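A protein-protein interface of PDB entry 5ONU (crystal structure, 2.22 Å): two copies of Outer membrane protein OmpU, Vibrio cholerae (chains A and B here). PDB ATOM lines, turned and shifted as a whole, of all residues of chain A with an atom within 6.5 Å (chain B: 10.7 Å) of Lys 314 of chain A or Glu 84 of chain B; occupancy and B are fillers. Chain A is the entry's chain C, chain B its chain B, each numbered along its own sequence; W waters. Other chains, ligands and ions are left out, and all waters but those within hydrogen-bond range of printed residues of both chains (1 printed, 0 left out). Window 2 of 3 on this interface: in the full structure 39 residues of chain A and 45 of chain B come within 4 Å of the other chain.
No position is printed for both chains.
Of the 7 pairs that touch across the chains among the printed residues, none has its exchanged pair printed and touching as well.
Of the 25 printed residues of chain B, 7 touch a printed residue of chain A.
Among the printed residues, 7 pairs touch across the chains.
Among the printed residues, no Asp or Glu carboxylate lies within 4 Å of a Lys or Arg side-chain nitrogen of the other chain.
Among the printed residues, pairs that only touch across the chains: Asn 316 of chain A with Thr 50 of chain B (3.5 Å), Phe 317 of chain A with Gly 121 of chain B (3.5 Å), Lys 314 of chain A with Glu 84 of chain B (3.5 Å), Phe 317 of chain A with Gly 91 of chain B (3.7 Å), Phe 317 of chain A with Ile 122 of chain B (3.7 Å), Phe 313 of chain A with Ile 85 of chain B (3.8 Å) and Phe 317 of chain A with Val 92 of chain B (3.9 Å).
The backbone carbonyl oxygen (O) of Val 92 of chain B sits at hydrogen-bond distance from the backbone NH (N) of Gly 121 of chain B (3.1 Å).
The backbone carbonyl oxygen (O) of Ala 83 of chain B is in hydrogen-bond range of the backbone NH (N) of Gly 91 of chain B (2.9 Å).
The backbone NH (N) of Glu 84 of chain B lies within hydrogen-bond range of the backbone carbonyl oxygen (O) of Gly 49 of chain B, 3.1 Å away.
Water W1 lies within hydrogen-bond range of the side-chain hydroxyl of Thr 50 of chain B (2.5 Å) and the side-chain amide oxygen of Asn 316 of chain A (2.9 Å).
Lys 314 of chain A touches just one residue of chain B: Glu 84.
No residue of chain B comes within 4 Å of Pro 315 of chain A.
Printed residues of chain B within 4 Å of Phe 317 of chain A: Gly 91 (3.7 Å), Val 92 (3.9 Å), Gly 121 (3.5 Å) and Ile 122 (3.7 Å).
Glu 84 of chain B touches just one residue of chain A: Lys 314 (3.5 Å).
Printed residues of chain A within 4 Å of Ile 122 of chain B: Phe 317 (3.7 Å).
The nearest residue of chain B that does not touch Lys 314 of chain A is Ile 85 of chain B (4.3 Å).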
ATOM      1  N   GLN A 284      21.408  39.096  16.031  1.00  0.00           N
ATOM      2  CA  GLN A 284      20.607  38.089  15.351  1.00  0.00           C
ATOM      3  C   GLN A 284      19.221  38.634  15.005  1.00  0.00           C
ATOM      4  O   GLN A 284      18.236  38.209  15.609  1.00  0.00           O
ATOM      5  CB  GLN A 284      20.473  36.837  16.225  1.00  0.00           C
ATOM      6  CG  GLN A 284      21.672  35.901  16.169  1.00  0.00           C
ATOM      7  CD  GLN A 284      21.750  34.980  17.373  1.00  0.00           C
ATOM      8  OE1 GLN A 284      20.736  34.657  17.989  1.00  0.00           O
ATOM      9  NE2 GLN A 284      22.962  34.567  17.723  1.00  0.00           N
ATOM     10  N   TYR A 311      14.125  36.589  12.522  1.00  0.00           N
ATOM     11  CA  TYR A 311      15.063  36.195  13.569  1.00  0.00           C
ATOM     12  C   TYR A 311      15.781  34.896  13.215  1.00  0.00           C
ATOM     13  O   TYR A 311      15.149  33.859  13.012  1.00  0.00           O
ATOM     14  CB  TYR A 311      14.344  36.043  14.914  1.00  0.00           C
ATOM     15  CG  TYR A 311      15.279  35.871  16.092  1.00  0.00           C
ATOM     16  CD1 TYR A 311      15.744  34.615  16.463  1.00  0.00           C
ATOM     17  CD2 TYR A 311      15.698  36.968  16.833  1.00  0.00           C
ATOM     18  CE1 TYR A 311      16.602  34.457  17.538  1.00  0.00           C
ATOM     19  CE2 TYR A 311      16.555  36.820  17.909  1.00  0.00           C
ATOM     20  CZ  TYR A 311      17.003  35.563  18.257  1.00  0.00           C
ATOM     21  OH  TYR A 311      17.854  35.412  19.328  1.00  0.00           O
ATOM     22  N   TYR A 312      17.106  34.963  13.148  1.00  0.00           N
ATOM     23  CA  TYR A 312      17.922  33.805  12.804  1.00  0.00           C
ATOM     24  C   TYR A 312      18.424  33.081  14.046  1.00  0.00           C
ATOM     25  O   TYR A 312      19.418  33.488  14.649  1.00  0.00           O
ATOM     26  CB  TYR A 312      19.105  34.219  11.923  1.00  0.00           C
ATOM     27  CG  TYR A 312      18.708  34.646  10.529  1.00  0.00           C
ATOM     28  CD1 TYR A 312      18.168  35.902  10.292  1.00  0.00           C
ATOM     29  CD2 TYR A 312      18.869  33.790   9.448  1.00  0.00           C
ATOM     30  CE1 TYR A 312      17.801  36.296   9.023  1.00  0.00           C
ATOM     31  CE2 TYR A 312      18.504  34.174   8.172  1.00  0.00           C
ATOM     32  CZ  TYR A 312      17.967  35.429   7.966  1.00  0.00           C
ATOM     33  OH  TYR A 312      17.603  35.825   6.701  1.00  0.00           O
ATOM     34  N   PHE A 313      17.728  32.016  14.430  1.00  0.00           N
ATOM     35  CA  PHE A 313      18.180  31.184  15.537  1.00  0.00           C
ATOM     36  C   PHE A 313      19.497  30.536  15.160  1.00  0.00           C
ATOM     37  O   PHE A 313      20.482  30.641  15.891  1.00  0.00           O
ATOM     38  CB  PHE A 313      17.150  30.110  15.882  1.00  0.00           C
ATOM     39  CG  PHE A 313      15.876  30.653  16.450  1.00  0.00           C
ATOM     40  CD1 PHE A 313      15.774  30.937  17.801  1.00  0.00           C
ATOM     41  CD2 PHE A 313      14.778  30.870  15.637  1.00  0.00           C
ATOM     42  CE1 PHE A 313      14.600  31.434  18.330  1.00  0.00           C
ATOM     43  CE2 PHE A 313      13.600  31.368  16.159  1.00  0.00           C
ATOM     44  CZ  PHE A 313      13.511  31.649  17.508  1.00  0.00           C
ATOM     45  N   LYS A 314      19.514  29.880  14.003  1.00  0.00           N
ATOM     46  CA  LYS A 314      20.750  29.303  13.490  1.00  0.00           C
ATOM     47  C   LYS A 314      20.853  29.664  12.010  1.00  0.00           C
ATOM     48  O   LYS A 314      19.854  30.071  11.414  1.00  0.00           O
ATOM     49  CB  LYS A 314      20.772  27.780  13.697  1.00  0.00           C
ATOM     50  CG  LYS A 314      20.663  27.328  15.154  1.00  0.00           C
ATOM     51  CD  LYS A 314      21.805  27.847  16.023  1.00  0.00           C
ATOM     52  CE  LYS A 314      23.020  26.935  15.990  1.00  0.00           C
ATOM     53  NZ  LYS A 314      23.897  27.163  17.176  1.00  0.00           N
ATOM     54  N   PRO A 315      22.050  29.512  11.408  1.00  0.00           N
ATOM     55  CA  PRO A 315      22.199  29.838   9.984  1.00  0.00           C
ATOM     56  C   PRO A 315      21.177  29.131   9.096  1.00  0.00           C
ATOM     57  O   PRO A 315      20.812  29.658   8.046  1.00  0.00           O
ATOM     58  CB  PRO A 315      23.616  29.359   9.666  1.00  0.00           C
ATOM     59  CG  PRO A 315      24.346  29.521  10.945  1.00  0.00           C
ATOM     60  CD  PRO A 315      23.350  29.197  12.030  1.00  0.00           C
ATOM     61  N   ASN A 316      20.721  27.956   9.520  1.00  0.00           N
ATOM     62  CA  ASN A 316      19.715  27.221   8.766  1.00  0.00           C
ATOM     63  C   ASN A 316      18.377  27.067   9.492  1.00  0.00           C
ATOM     64  O   ASN A 316      17.611  26.152   9.189  1.00  0.00           O
ATOM     65  CB  ASN A 316      20.251  25.838   8.394  1.00  0.00           C
ATOM     66  CG  ASN A 316      20.510  24.965   9.608  1.00  0.00           C
ATOM     67  OD1 ASN A 316      20.615  25.457  10.733  1.00  0.00           O
ATOM     68  ND2 ASN A 316      20.610  23.661   9.386  1.00  0.00           N
ATOM     69  N   PHE A 317      18.090  27.954  10.440  1.00  0.00           N
ATOM     70  CA  PHE A 317      16.767  27.960  11.059  1.00  0.00           C
ATOM     71  C   PHE A 317      16.357  29.357  11.498  1.00  0.00           C
ATOM     72  O   PHE A 317      17.046  29.996  12.313  1.00  0.00           O
ATOM     73  CB  PHE A 317      16.705  27.007  12.253  1.00  0.00           C
ATOM     74  CG  PHE A 317      15.318  26.832  12.805  1.00  0.00           C
ATOM     75  CD1 PHE A 317      14.385  26.066  12.123  1.00  0.00           C
ATOM     76  CD2 PHE A 317      14.941  27.439  13.991  1.00  0.00           C
ATOM     77  CE1 PHE A 317      13.104  25.904  12.616  1.00  0.00           C
ATOM     78  CE2 PHE A 317      13.660  27.279  14.490  1.00  0.00           C
ATOM     79  CZ  PHE A 317      12.741  26.511  13.801  1.00  0.00           C
ATOM     80  N   ARG A 318      15.222  29.810  10.958  1.00  0.00           N
ATOM     81  CA  ARG A 318      14.765  31.185  11.146  1.00  0.00           C
ATOM     82  C   ARG A 318      13.241  31.280  11.250  1.00  0.00           C
ATOM     83  O   ARG A 318      12.525  30.401  10.778  1.00  0.00           O
ATOM     84  CB  ARG A 318      15.253  32.060   9.990  1.00  0.00           C
ATOM     85  CG  ARG A 318      14.459  31.866   8.705  1.00  0.00           C
ATOM     86  CD  ARG A 318      15.103  32.565   7.522  1.00  0.00           C
ATOM     87  NE  ARG A 318      16.243  31.809   7.012  1.00  0.00           N
ATOM     88  CZ  ARG A 318      16.865  32.072   5.867  1.00  0.00           C
ATOM     89  NH1 ARG A 318      16.456  33.076   5.103  1.00  0.00           N
ATOM     90  NH2 ARG A 318      17.894  31.328   5.482  1.00  0.00           N
ATOM     91  N   TYR B  45      24.733  13.625   6.836  1.00  0.00           N
ATOM     92  CA  TYR B  45      25.666  14.645   7.290  1.00  0.00           C
ATOM     93  C   TYR B  45      25.258  15.139   8.665  1.00  0.00           C
ATOM     94  O   TYR B  45      24.072  15.172   8.998  1.00  0.00           O
ATOM     95  CB  TYR B  45      25.716  15.817   6.296  1.00  0.00           C
ATOM     96  CG  TYR B  45      26.027  17.167   6.921  1.00  0.00           C
ATOM     97  CD1 TYR B  45      27.338  17.584   7.114  1.00  0.00           C
ATOM     98  CD2 TYR B  45      25.004  18.026   7.313  1.00  0.00           C
ATOM     99  CE1 TYR B  45      27.622  18.816   7.686  1.00  0.00           C
ATOM    100  CE2 TYR B  45      25.278  19.256   7.887  1.00  0.00           C
ATOM    101  CZ  TYR B  45      26.588  19.647   8.069  1.00  0.00           C
ATOM    102  OH  TYR B  45      26.859  20.870   8.637  1.00  0.00           O
ATOM    103  N   SER B  46      26.244  15.539   9.460  1.00  0.00           N
ATOM    104  CA  SER B  46      25.966  16.139  10.755  1.00  0.00           C
ATOM    105  C   SER B  46      27.155  16.953  11.236  1.00  0.00           C
ATOM    106  O   SER B  46      28.303  16.648  10.901  1.00  0.00           O
ATOM    107  CB  SER B  46      25.617  15.063  11.786  1.00  0.00           C
ATOM    108  OG  SER B  46      26.649  14.099  11.887  1.00  0.00           O
ATOM    109  N   ALA B  47      26.870  17.974  12.038  1.00  0.00           N
ATOM    110  CA  ALA B  47      27.908  18.851  12.569  1.00  0.00           C
ATOM    111  C   ALA B  47      27.382  19.787  13.654  1.00  0.00           C
ATOM    112  O   ALA B  47      26.458  20.567  13.418  1.00  0.00           O
ATOM    113  CB  ALA B  47      28.542  19.662  11.446  1.00  0.00           C
ATOM    114  N   LYS B  48      27.979  19.697  14.840  1.00  0.00           N
ATOM    115  CA  LYS B  48      27.759  20.657  15.926  1.00  0.00           C
ATOM    116  C   LYS B  48      26.287  20.852  16.321  1.00  0.00           C
ATOM    117  O   LYS B  48      25.846  21.982  16.532  1.00  0.00           O
ATOM    118  CB  LYS B  48      28.377  22.033  15.570  1.00  0.00           C
ATOM    119  CG  LYS B  48      29.919  22.145  15.366  1.00  0.00           C
ATOM    120  CD  LYS B  48      30.647  20.874  14.951  1.00  0.00           C
ATOM    121  CE  LYS B  48      32.085  21.113  14.543  1.00  0.00           C
ATOM    122  NZ  LYS B  48      32.639  19.887  13.905  1.00  0.00           N
ATOM    123  N   GLY B  49      25.532  19.759  16.431  1.00  0.00           N
ATOM    124  CA  GLY B  49      24.140  19.849  16.848  1.00  0.00           C
ATOM    125  C   GLY B  49      23.124  19.806  15.724  1.00  0.00           C
ATOM    126  O   GLY B  49      21.919  19.735  15.969  1.00  0.00           O
ATOM    127  N   THR B  50      23.610  19.840  14.490  1.00  0.00           N
ATOM    128  CA  THR B  50      22.735  19.863  13.325  1.00  0.00           C
ATOM    129  C   THR B  50      22.918  18.627  12.452  1.00  0.00           C
ATOM    130  O   THR B  50      24.040  18.277  12.093  1.00  0.00           O
ATOM    131  CB  THR B  50      22.991  21.119  12.474  1.00  0.00           C
ATOM    132  OG1 THR B  50      22.776  22.290  13.271  1.00  0.00           O
ATOM    133  CG2 THR B  50      22.066  21.149  11.266  1.00  0.00           C
ATOM    134  N   SER B  51      21.814  17.966  12.112  1.00  0.00           N
ATOM    135  CA  SER B  51      21.888  16.770  11.279  1.00  0.00           C
ATOM    136  C   SER B  51      20.779  16.656  10.232  1.00  0.00           C
ATOM    137  O   SER B  51      19.726  17.300  10.336  1.00  0.00           O
ATOM    138  CB  SER B  51      21.868  15.521  12.164  1.00  0.00           C
ATOM    139  OG  SER B  51      20.693  15.482  12.958  1.00  0.00           O
ATOM    140  N   LEU B  52      21.040  15.817   9.231  1.00  0.00           N
ATOM    141  CA  LEU B  52      20.062  15.442   8.217  1.00  0.00           C
ATOM    142  C   LEU B  52      20.024  13.926   8.040  1.00  0.00           C
ATOM    143  O   LEU B  52      21.057  13.277   7.826  1.00  0.00           O
ATOM    144  CB  LEU B  52      20.370  16.112   6.877  1.00  0.00           C
ATOM    145  CG  LEU B  52      19.405  15.734   5.746  1.00  0.00           C
ATOM    146  CD1 LEU B  52      18.006  16.275   6.010  1.00  0.00           C
ATOM    147  CD2 LEU B  52      19.925  16.201   4.393  1.00  0.00           C
ATOM    148  N   GLY B  81      15.550  17.108   8.955  1.00  0.00           N
ATOM    149  CA  GLY B  81      16.592  17.984   9.461  1.00  0.00           C
ATOM    150  C   GLY B  81      16.337  18.428  10.888  1.00  0.00           C
ATOM    151  O   GLY B  81      15.205  18.755  11.247  1.00  0.00           O
ATOM    152  N   LYS B  82      17.383  18.440  11.711  1.00  0.00           N
ATOM    153  CA  LYS B  82      17.237  18.891  13.094  1.00  0.00           C
ATOM    154  C   LYS B  82      18.425  19.742  13.533  1.00  0.00           C
ATOM    155  O   LYS B  82      19.579  19.361  13.339  1.00  0.00           O
ATOM    156  CB  LYS B  82      17.069  17.703  14.042  1.00  0.00           C
ATOM    157  CG  LYS B  82      16.770  18.108  15.481  1.00  0.00           C
ATOM    158  CD  LYS B  82      16.397  16.911  16.345  1.00  0.00           C
ATOM    159  CE  LYS B  82      16.293  17.308  17.811  1.00  0.00           C
ATOM    160  NZ  LYS B  82      16.026  16.138  18.694  1.00  0.00           N
ATOM    161  N   ALA B  83      18.131  20.898  14.122  1.00  0.00           N
ATOM    162  CA  ALA B  83      19.165  21.842  14.533  1.00  0.00           C
ATOM    163  C   ALA B  83      18.991  22.288  15.984  1.00  0.00           C
ATOM    164  O   ALA B  83      17.974  22.886  16.338  1.00  0.00           O
ATOM    165  CB  ALA B  83      19.175  23.053  13.608  1.00  0.00           C
ATOM    166  N   GLU B  84      19.984  21.996  16.818  1.00  0.00           N
ATOM    167  CA  GLU B  84      19.965  22.445  18.206  1.00  0.00           C
ATOM    168  C   GLU B  84      20.195  23.953  18.289  1.00  0.00           C
ATOM    169  O   GLU B  84      21.100  24.489  17.650  1.00  0.00           O
ATOM    170  CB  GLU B  84      21.025  21.703  19.033  1.00  0.00           C
ATOM    171  CG  GLU B  84      21.658  22.543  20.144  1.00  0.00           C
ATOM    172  CD  GLU B  84      22.657  21.767  20.990  1.00  0.00           C
ATOM    173  OE1 GLU B  84      22.937  20.591  20.674  1.00  0.00           O
ATOM    174  OE2 GLU B  84      23.169  22.343  21.973  1.00  0.00           O
ATOM    175  N   ILE B  85      19.358  24.638  19.063  1.00  0.00           N
ATOM    176  CA  ILE B  85      19.527  26.067  19.290  1.00  0.00           C
ATOM    177  C   ILE B  85      20.220  26.236  20.635  1.00  0.00           C
ATOM    178  O   ILE B  85      21.223  26.943  20.750  1.00  0.00           O
ATOM    179  CB  ILE B  85      18.194  26.821  19.272  1.00  0.00           C
ATOM    180  CG1 ILE B  85      17.476  26.584  17.944  1.00  0.00           C
ATOM    181  CG2 ILE B  85      18.426  28.306  19.492  1.00  0.00           C
ATOM    182  CD1 ILE B  85      16.064  27.128  17.903  1.00  0.00           C
ATOM    183  N   ASN B  86      19.674  25.577  21.652  1.00  0.00           N
ATOM    184  CA  ASN B  86      20.392  25.394  22.904  1.00  0.00           C
ATOM    185  C   ASN B  86      19.966  24.088  23.558  1.00  0.00           C
ATOM    186  O   ASN B  86      19.178  23.329  22.988  1.00  0.00           O
ATOM    187  CB  ASN B  86      20.168  26.581  23.850  1.00  0.00           C
ATOM    188  CG  ASN B  86      18.704  26.795  24.198  1.00  0.00           C
ATOM    189  OD1 ASN B  86      18.045  25.913  24.751  1.00  0.00           O
ATOM    190  ND2 ASN B  86      18.189  27.975  23.878  1.00  0.00           N
ATOM    191  N   ASP B  87      20.439  23.860  24.779  1.00  0.00           N
ATOM    192  CA  ASP B  87      20.304  22.560  25.428  1.00  0.00           C
ATOM    193  C   ASP B  87      18.846  22.200  25.704  1.00  0.00           C
ATOM    194  O   ASP B  87      18.534  21.060  26.047  1.00  0.00           O
ATOM    195  CB  ASP B  87      21.109  22.528  26.727  1.00  0.00           C
ATOM    196  CG  ASP B  87      21.647  21.146  27.046  1.00  0.00           C
ATOM    197  OD1 ASP B  87      21.137  20.159  26.475  1.00  0.00           O
ATOM    198  OD2 ASP B  87      22.582  21.045  27.867  1.00  0.00           O
ATOM    199  N   SER B  88      17.955  23.173  25.551  1.00  0.00           N
ATOM    200  CA  SER B  88      16.537  22.941  25.774  1.00  0.00           C
ATOM    201  C   SER B  88      15.691  23.516  24.643  1.00  0.00           C
ATOM    202  O   SER B  88      14.503  23.783  24.828  1.00  0.00           O
ATOM    203  CB  SER B  88      16.100  23.543  27.112  1.00  0.00           C
ATOM    204  OG  SER B  88      16.262  24.950  27.117  1.00  0.00           O
ATOM    205  N   LEU B  89      16.297  23.706  23.472  1.00  0.00           N
ATOM    206  CA  LEU B  89      15.564  24.275  22.343  1.00  0.00           C
ATOM    207  C   LEU B  89      16.167  23.875  20.996  1.00  0.00           C
ATOM    208  O   LEU B  89      17.379  23.979  20.792  1.00  0.00           O
ATOM    209  CB  LEU B  89      15.513  25.799  22.464  1.00  0.00           C
ATOM    210  CG  LEU B  89      14.538  26.520  21.533  1.00  0.00           C
ATOM    211  CD1 LEU B  89      13.105  26.132  21.862  1.00  0.00           C
ATOM    212  CD2 LEU B  89      14.722  28.025  21.632  1.00  0.00           C
ATOM    213  N   TYR B  90      15.308  23.430  20.078  1.00  0.00           N
ATOM    214  CA  TYR B  90      15.737  23.001  18.748  1.00  0.00           C
ATOM    215  C   TYR B  90      14.706  23.336  17.667  1.00  0.00           C
ATOM    216  O   TYR B  90      13.537  23.584  17.966  1.00  0.00           O
ATOM    217  CB  TYR B  90      16.018  21.495  18.734  1.00  0.00           C
ATOM    218  CG  TYR B  90      14.796  20.638  18.988  1.00  0.00           C
ATOM    219  CD1 TYR B  90      14.039  20.145  17.932  1.00  0.00           C
ATOM    220  CD2 TYR B  90      14.401  20.319  20.280  1.00  0.00           C
ATOM    221  CE1 TYR B  90      12.922  19.363  18.155  1.00  0.00           C
ATOM    222  CE2 TYR B  90      13.286  19.536  20.513  1.00  0.00           C
ATOM    223  CZ  TYR B  90      12.550  19.061  19.447  1.00  0.00           C
ATOM    224  OH  TYR B  90      11.439  18.282  19.674  1.00  0.00           O
ATOM    225  N   GLY B  91      15.153  23.346  16.413  1.00  0.00           N
ATOM    226  CA  GLY B  91      14.269  23.504  15.266  1.00  0.00           C
ATOM    227  C   GLY B  91      14.224  22.246  14.412  1.00  0.00           C
ATOM    228  O   GLY B  91      15.133  21.418  14.480  1.00  0.00           O
ATOM    229  N   VAL B  92      13.175  22.098  13.604  1.00  0.00           N
ATOM    230  CA  VAL B  92      12.979  20.867  12.835  1.00  0.00           C
ATOM    231  C   VAL B  92      12.285  21.108  11.482  1.00  0.00           C
ATOM    232  O   VAL B  92      11.441  21.996  11.353  1.00  0.00           O
ATOM    233  CB  VAL B  92      12.166  19.835  13.664  1.00  0.00           C
ATOM    234  CG1 VAL B  92      10.762  20.352  13.948  1.00  0.00           C
ATOM    235  CG2 VAL B  92      12.119  18.481  12.969  1.00  0.00           C
ATOM    236  N   GLY B  93      12.664  20.321  10.475  1.00  0.00           N
ATOM    237  CA  GLY B  93      12.022  20.346   9.169  1.00  0.00           C
ATOM    238  C   GLY B  93      11.900  18.952   8.570  1.00  0.00           C
ATOM    239  O   GLY B  93      12.835  18.155   8.659  1.00  0.00           O
ATOM    240  N   GLY B 121       8.767  23.191  12.453  1.00  0.00           N
ATOM    241  CA  GLY B 121       8.378  23.357  13.841  1.00  0.00           C
ATOM    242  C   GLY B 121       9.479  23.688  14.831  1.00  0.00           C
ATOM    243  O   GLY B 121      10.654  23.793  14.473  1.00  0.00           O
ATOM    244  N   ILE B 122       9.078  23.855  16.089  1.00  0.00           N
ATOM    245  CA  ILE B 122       9.994  24.179  17.179  1.00  0.00           C
ATOM    246  C   ILE B 122       9.666  23.316  18.397  1.00  0.00           C
ATOM    247  O   ILE B 122       8.496  23.024  18.666  1.00  0.00           O
ATOM    248  CB  ILE B 122       9.918  25.675  17.583  1.00  0.00           C
ATOM    249  CG1 ILE B 122      10.002  26.583  16.356  1.00  0.00           C
ATOM    250  CG2 ILE B 122      11.019  26.027  18.575  1.00  0.00           C
ATOM    251  CD1 ILE B 122      10.071  28.059  16.697  1.00  0.00           C
ATOM    252  N   GLY B 123      10.699  22.897  19.122  1.00  0.00           N
ATOM    253  CA  GLY B 123      10.507  22.048  20.282  1.00  0.00           C
ATOM    254  C   GLY B 123      11.518  22.230  21.400  1.00  0.00           C
ATOM    255  O   GLY B 123      12.530  22.915  21.244  1.00  0.00           O
ATOM    256  N   GLY B 124      11.227  21.605  22.536  1.00  0.00           N
ATOM    257  CA  GLY B 124      12.110  21.606  23.686  1.00  0.00           C
ATOM    258  C   GLY B 124      11.442  20.962  24.887  1.00  0.00           C
ATOM    259  O   GLY B 124      10.650  20.028  24.741  1.00  0.00           O
HETATM  260  O   HOH W   1      22.537  24.689  12.739  1.00  0.00           O
